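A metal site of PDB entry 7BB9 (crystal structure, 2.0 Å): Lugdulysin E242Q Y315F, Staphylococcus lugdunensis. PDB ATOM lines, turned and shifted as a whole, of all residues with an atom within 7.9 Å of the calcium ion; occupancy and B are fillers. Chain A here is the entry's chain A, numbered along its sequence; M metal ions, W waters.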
ATOM      1  N   ASN A 221      16.784 -25.189 -14.966  1.00  0.00           N
ATOM      2  CA  ASN A 221      18.244 -25.093 -15.031  1.00  0.00           C
ATOM      3  C   ASN A 221      18.838 -26.385 -15.566  1.00  0.00           C
ATOM      4  O   ASN A 221      19.665 -26.384 -16.492  1.00  0.00           O
ATOM      5  CB  ASN A 221      18.801 -24.787 -13.645  1.00  0.00           C
ATOM      6  CG  ASN A 221      20.209 -24.229 -13.685  1.00  0.00           C
ATOM      7  OD1 ASN A 221      21.102 -24.821 -14.303  1.00  0.00           O
ATOM      8  ND2 ASN A 221      20.418 -23.106 -13.012  1.00  0.00           N
ATOM      9  N   GLU A 224      18.001 -26.728 -19.427  1.00  0.00           N
ATOM     10  CA  GLU A 224      18.773 -25.889 -20.333  1.00  0.00           C
ATOM     11  C   GLU A 224      20.199 -26.388 -20.462  1.00  0.00           C
ATOM     12  O   GLU A 224      20.737 -26.479 -21.570  1.00  0.00           O
ATOM     13  CB  GLU A 224      18.750 -24.430 -19.855  1.00  0.00           C
ATOM     14  CG  GLU A 224      17.369 -23.798 -19.816  1.00  0.00           C
ATOM     15  CD  GLU A 224      16.863 -23.421 -21.199  1.00  0.00           C
ATOM     16  OE1 GLU A 224      17.684 -23.306 -22.135  1.00  0.00           O
ATOM     17  OE2 GLU A 224      15.643 -23.250 -21.347  1.00  0.00           O
ATOM     18  N   ASN A 225      20.811 -26.773 -19.342  1.00  0.00           N
ATOM     19  CA  ASN A 225      22.233 -27.107 -19.348  1.00  0.00           C
ATOM     20  C   ASN A 225      22.523 -28.560 -19.669  1.00  0.00           C
ATOM     21  O   ASN A 225      23.579 -28.855 -20.244  1.00  0.00           O
ATOM     22  CB  ASN A 225      22.868 -26.734 -18.004  1.00  0.00           C
ATOM     23  CG  ASN A 225      23.012 -25.229 -17.830  1.00  0.00           C
ATOM     24  OD1 ASN A 225      23.632 -24.551 -18.646  1.00  0.00           O
ATOM     25  ND2 ASN A 225      22.439 -24.689 -16.750  1.00  0.00           N
ATOM     26  N   LEU A 226      21.615 -29.495 -19.357  1.00  0.00           N
ATOM     27  CA  LEU A 226      21.890 -30.901 -19.649  1.00  0.00           C
ATOM     28  C   LEU A 226      21.247 -31.387 -20.943  1.00  0.00           C
ATOM     29  O   LEU A 226      21.759 -32.337 -21.540  1.00  0.00           O
ATOM     30  CB  LEU A 226      21.430 -31.799 -18.491  1.00  0.00           C
ATOM     31  CG  LEU A 226      22.094 -31.459 -17.156  1.00  0.00           C
ATOM     32  CD1 LEU A 226      21.577 -32.357 -16.065  1.00  0.00           C
ATOM     33  CD2 LEU A 226      23.599 -31.555 -17.259  1.00  0.00           C
ATOM     34  N   GLU A 229      21.897 -27.641 -24.264  1.00  0.00           N
ATOM     35  CA  GLU A 229      23.261 -27.273 -24.605  1.00  0.00           C
ATOM     36  C   GLU A 229      24.104 -28.527 -24.803  1.00  0.00           C
ATOM     37  O   GLU A 229      23.923 -29.523 -24.107  1.00  0.00           O
ATOM     38  CB  GLU A 229      23.873 -26.389 -23.510  1.00  0.00           C
ATOM     39  CG  GLU A 229      23.232 -25.006 -23.418  1.00  0.00           C
ATOM     40  CD  GLU A 229      23.664 -24.287 -22.168  1.00  0.00           C
ATOM     41  OE1 GLU A 229      22.917 -23.391 -21.719  1.00  0.00           O
ATOM     42  OE2 GLU A 229      24.746 -24.625 -21.628  1.00  0.00           O
ATOM     43  N   SER A 231      27.316 -29.150 -24.311  1.00  0.00           N
ATOM     44  CA  SER A 231      28.374 -29.501 -23.347  1.00  0.00           C
ATOM     45  C   SER A 231      27.849 -30.346 -22.194  1.00  0.00           C
ATOM     46  O   SER A 231      28.624 -31.114 -21.592  1.00  0.00           O
ATOM     47  CB  SER A 231      29.066 -28.238 -22.816  1.00  0.00           C
ATOM     48  OG  SER A 231      28.170 -27.140 -22.696  1.00  0.00           O
ATOM     49  N   GLU A 233      27.073 -29.604 -19.164  1.00  0.00           N
ATOM     50  CA  GLU A 233      27.761 -29.253 -17.934  1.00  0.00           C
ATOM     51  C   GLU A 233      26.769 -28.680 -16.921  1.00  0.00           C
ATOM     52  O   GLU A 233      26.139 -27.661 -17.187  1.00  0.00           O
ATOM     53  CB  GLU A 233      28.876 -28.239 -18.203  1.00  0.00           C
ATOM     54  CG  GLU A 233      30.236 -28.850 -18.449  1.00  0.00           C
ATOM     55  CD  GLU A 233      31.329 -27.797 -18.478  1.00  0.00           C
ATOM     56  OE1 GLU A 233      31.863 -27.483 -17.389  1.00  0.00           O
ATOM     57  OE2 GLU A 233      31.633 -27.278 -19.573  1.00  0.00           O
ATOM     58  N   GLU A 234      26.639 -29.351 -15.779  1.00  0.00           N
ATOM     59  CA  GLU A 234      25.876 -28.794 -14.668  1.00  0.00           C
ATOM     60  C   GLU A 234      26.491 -27.480 -14.193  1.00  0.00           C
ATOM     61  O   GLU A 234      27.708 -27.336 -14.089  1.00  0.00           O
ATOM     62  CB  GLU A 234      25.868 -29.766 -13.489  1.00  0.00           C
ATOM     63  CG  GLU A 234      24.744 -30.770 -13.468  1.00  0.00           C
ATOM     64  CD  GLU A 234      24.871 -31.726 -12.291  1.00  0.00           C
ATOM     65  OE1 GLU A 234      26.027 -32.096 -11.964  1.00  0.00           O
ATOM     66  OE2 GLU A 234      23.832 -32.113 -11.701  1.00  0.00           O
ATOM     67  N   MET A 235      25.621 -26.540 -13.840  1.00  0.00           N
ATOM     68  CA  MET A 235      26.032 -25.374 -13.076  1.00  0.00           C
ATOM     69  C   MET A 235      26.488 -25.795 -11.687  1.00  0.00           C
ATOM     70  O   MET A 235      25.927 -26.730 -11.096  1.00  0.00           O
ATOM     71  CB  MET A 235      24.869 -24.387 -12.954  1.00  0.00           C
ATOM     72  CG  MET A 235      25.254 -22.981 -12.566  1.00  0.00           C
ATOM     73  SD  MET A 235      23.797 -21.925 -12.569  1.00  0.00           S
ATOM     74  CE  MET A 235      23.566 -21.609 -14.336  1.00  0.00           C
ATOM     75  N   LYS A 310      18.741 -14.936 -16.922  1.00  0.00           N
ATOM     76  CA  LYS A 310      18.560 -15.907 -18.005  1.00  0.00           C
ATOM     77  C   LYS A 310      19.820 -15.999 -18.864  1.00  0.00           C
ATOM     78  O   LYS A 310      20.083 -17.060 -19.443  1.00  0.00           O
ATOM     79  CB  LYS A 310      17.343 -15.539 -18.872  1.00  0.00           C
ATOM     80  CG  LYS A 310      17.477 -14.219 -19.615  1.00  0.00           C
ATOM     81  CD  LYS A 310      16.733 -14.248 -20.934  1.00  0.00           C
ATOM     82  CE  LYS A 310      15.224 -14.139 -20.726  1.00  0.00           C
ATOM     83  NZ  LYS A 310      14.770 -12.727 -20.564  1.00  0.00           N
ATOM     84  N   GLU A 311      20.605 -14.923 -18.938  1.00  0.00           N
ATOM     85  CA  GLU A 311      21.874 -14.991 -19.650  1.00  0.00           C
ATOM     86  C   GLU A 311      22.866 -15.911 -18.962  1.00  0.00           C
ATOM     87  O   GLU A 311      23.689 -16.553 -19.634  1.00  0.00           O
ATOM     88  CB  GLU A 311      22.472 -13.580 -19.804  1.00  0.00           C
ATOM     89  CG  GLU A 311      21.579 -12.632 -20.554  1.00  0.00           C
ATOM     90  CD  GLU A 311      22.256 -11.319 -20.852  1.00  0.00           C
ATOM     91  OE1 GLU A 311      21.569 -10.275 -20.793  1.00  0.00           O
ATOM     92  OE2 GLU A 311      23.478 -11.311 -21.140  1.00  0.00           O
ATOM     93  N   LEU A 312      22.838 -15.975 -17.625  1.00  0.00           N
ATOM     94  CA  LEU A 312      23.749 -16.901 -16.952  1.00  0.00           C
ATOM     95  C   LEU A 312      23.414 -18.344 -17.303  1.00  0.00           C
ATOM     96  O   LEU A 312      24.320 -19.161 -17.514  1.00  0.00           O
ATOM     97  CB  LEU A 312      23.697 -16.709 -15.436  1.00  0.00           C
ATOM     98  CG  LEU A 312      24.334 -15.496 -14.732  1.00  0.00           C
ATOM     99  CD1 LEU A 312      24.065 -15.589 -13.235  1.00  0.00           C
ATOM    100  CD2 LEU A 312      25.837 -15.430 -15.000  1.00  0.00           C
ATOM    101  N   ILE A 313      22.126 -18.671 -17.353  1.00  0.00           N
ATOM    102  CA  ILE A 313      21.712 -20.020 -17.726  1.00  0.00           C
ATOM    103  C   ILE A 313      22.009 -20.295 -19.202  1.00  0.00           C
ATOM    104  O   ILE A 313      22.526 -21.351 -19.554  1.00  0.00           O
ATOM    105  CB  ILE A 313      20.213 -20.213 -17.418  1.00  0.00           C
ATOM    106  CG1 ILE A 313      19.950 -20.045 -15.928  1.00  0.00           C
ATOM    107  CG2 ILE A 313      19.725 -21.584 -17.901  1.00  0.00           C
ATOM    108  CD1 ILE A 313      18.460 -20.192 -15.567  1.00  0.00           C
ATOM    109  N   ASN A 314      21.674 -19.344 -20.072  1.00  0.00           N
ATOM    110  CA  ASN A 314      21.826 -19.535 -21.504  1.00  0.00           C
ATOM    111  C   ASN A 314      23.281 -19.604 -21.956  1.00  0.00           C
ATOM    112  O   ASN A 314      23.541 -20.088 -23.068  1.00  0.00           O
ATOM    113  CB  ASN A 314      21.124 -18.419 -22.268  1.00  0.00           C
ATOM    114  CG  ASN A 314      19.673 -18.709 -22.490  1.00  0.00           C
ATOM    115  OD1 ASN A 314      19.281 -19.861 -22.640  1.00  0.00           O
ATOM    116  ND2 ASN A 314      18.856 -17.665 -22.504  1.00  0.00           N
ATOM    117  N   ASP A 315      24.215 -19.120 -21.157  1.00  0.00           N
ATOM    118  CA  ASP A 315      25.617 -19.170 -21.561  1.00  0.00           C
ATOM    119  C   ASP A 315      26.068 -20.629 -21.691  1.00  0.00           C
ATOM    120  O   ASP A 315      25.757 -21.453 -20.822  1.00  0.00           O
ATOM    121  CB  ASP A 315      26.505 -18.446 -20.546  1.00  0.00           C
ATOM    122  CG  ASP A 315      27.835 -18.036 -21.139  1.00  0.00           C
ATOM    123  OD1 ASP A 315      28.670 -18.925 -21.409  1.00  0.00           O
ATOM    124  OD2 ASP A 315      28.034 -16.813 -21.349  1.00  0.00           O
ATOM    125  N   PRO A 316      26.784 -20.982 -22.751  1.00  0.00           N
ATOM    126  CA  PRO A 316      27.144 -22.390 -22.965  1.00  0.00           C
ATOM    127  C   PRO A 316      28.376 -22.853 -22.207  1.00  0.00           C
ATOM    128  O   PRO A 316      28.606 -24.066 -22.143  1.00  0.00           O
ATOM    129  CB  PRO A 316      27.376 -22.466 -24.472  1.00  0.00           C
ATOM    130  CG  PRO A 316      27.853 -21.090 -24.822  1.00  0.00           C
ATOM    131  CD  PRO A 316      27.101 -20.141 -23.915  1.00  0.00           C
ATOM    132  N   GLY A 317      29.173 -21.928 -21.643  1.00  0.00           N
ATOM    133  CA  GLY A 317      30.362 -22.303 -20.900  1.00  0.00           C
ATOM    134  C   GLY A 317      30.060 -22.665 -19.443  1.00  0.00           C
ATOM    135  O   GLY A 317      28.924 -22.587 -18.976  1.00  0.00           O
ATOM    136  N   ASP A 318      31.112 -23.073 -18.736  1.00  0.00           N
ATOM    137  CA  ASP A 318      30.943 -23.508 -17.359  1.00  0.00           C
ATOM    138  C   ASP A 318      30.623 -22.324 -16.461  1.00  0.00           C
ATOM    139  O   ASP A 318      30.508 -21.175 -16.917  1.00  0.00           O
ATOM    140  CB  ASP A 318      32.180 -24.286 -16.867  1.00  0.00           C
ATOM    141  CG  ASP A 318      33.469 -23.446 -16.874  1.00  0.00           C
ATOM    142  OD1 ASP A 318      33.412 -22.205 -16.995  1.00  0.00           O
ATOM    143  OD2 ASP A 318      34.568 -24.045 -16.744  1.00  0.00           O
ATOM    144  N   THR A 319      30.490 -22.601 -15.165  1.00  0.00           N
ATOM    145  CA  THR A 319      29.867 -21.647 -14.239  1.00  0.00           C
ATOM    146  C   THR A 319      30.677 -20.370 -14.134  1.00  0.00           C
ATOM    147  O   THR A 319      30.129 -19.259 -14.163  1.00  0.00           O
ATOM    148  CB  THR A 319      29.704 -22.305 -12.861  1.00  0.00           C
ATOM    149  OG1 THR A 319      28.734 -23.357 -12.944  1.00  0.00           O
ATOM    150  CG2 THR A 319      29.254 -21.307 -11.833  1.00  0.00           C
ATOM    151  N   ALA A 322      30.460 -18.328 -17.447  1.00  0.00           N
ATOM    152  CA  ALA A 322      29.191 -17.607 -17.591  1.00  0.00           C
ATOM    153  C   ALA A 322      29.176 -16.334 -16.748  1.00  0.00           C
ATOM    154  O   ALA A 322      28.787 -15.258 -17.222  1.00  0.00           O
ATOM    155  CB  ALA A 322      28.024 -18.510 -17.206  1.00  0.00           C
HETATM  156 CA    CA M   1      24.344 -22.804 -19.840  1.00  0.00          CA
HETATM  157  O   HOH W   1      26.417 -24.005 -19.347  1.00  0.00           O
HETATM  158  O   HOH W   2      24.835 -21.679 -17.806  1.00  0.00           O
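The calcium ion is bound by the backbone carbonyl oxygen (O) of Asp 315 (2.2 Å), the side-chain amide oxygen (OD1) of Asn 225 (2.2 Å), the backbone carbonyl oxygen (O) of Ile 313 (2.3 Å), water W2 (2.4 Å), the side-chain carboxylate (OE1) of Glu 229 (2.4 Å), water W1 (2.4 Å) and the side-chain carboxylate (OE2) of Glu 229 (2.6 Å).
Residues that only touch the calcium ion: Asn 314 (3.98 Å). Of the 20 residues printed, 5 come within 4 Å of the calcium ion.
ND2 of Asn 225 sits at hydrogen-bond distance from OD1 of Asn 221, at 2.8 Å. The backbone carbonyl oxygen (O) of Lys 310 sits close to the side-chain amide nitrogen (ND2) of Asn 314, 3.4 Å away. The side-chain carboxylate of Asp 315 lies within hydrogen-bond range of the backbone NH of Gly 317 (3.1 Å). The backbone carbonyl oxygen (O) of Glu 224 sits at hydrogen-bond distance from the backbone NH (N) of Glu 229, 3.2 Å away.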
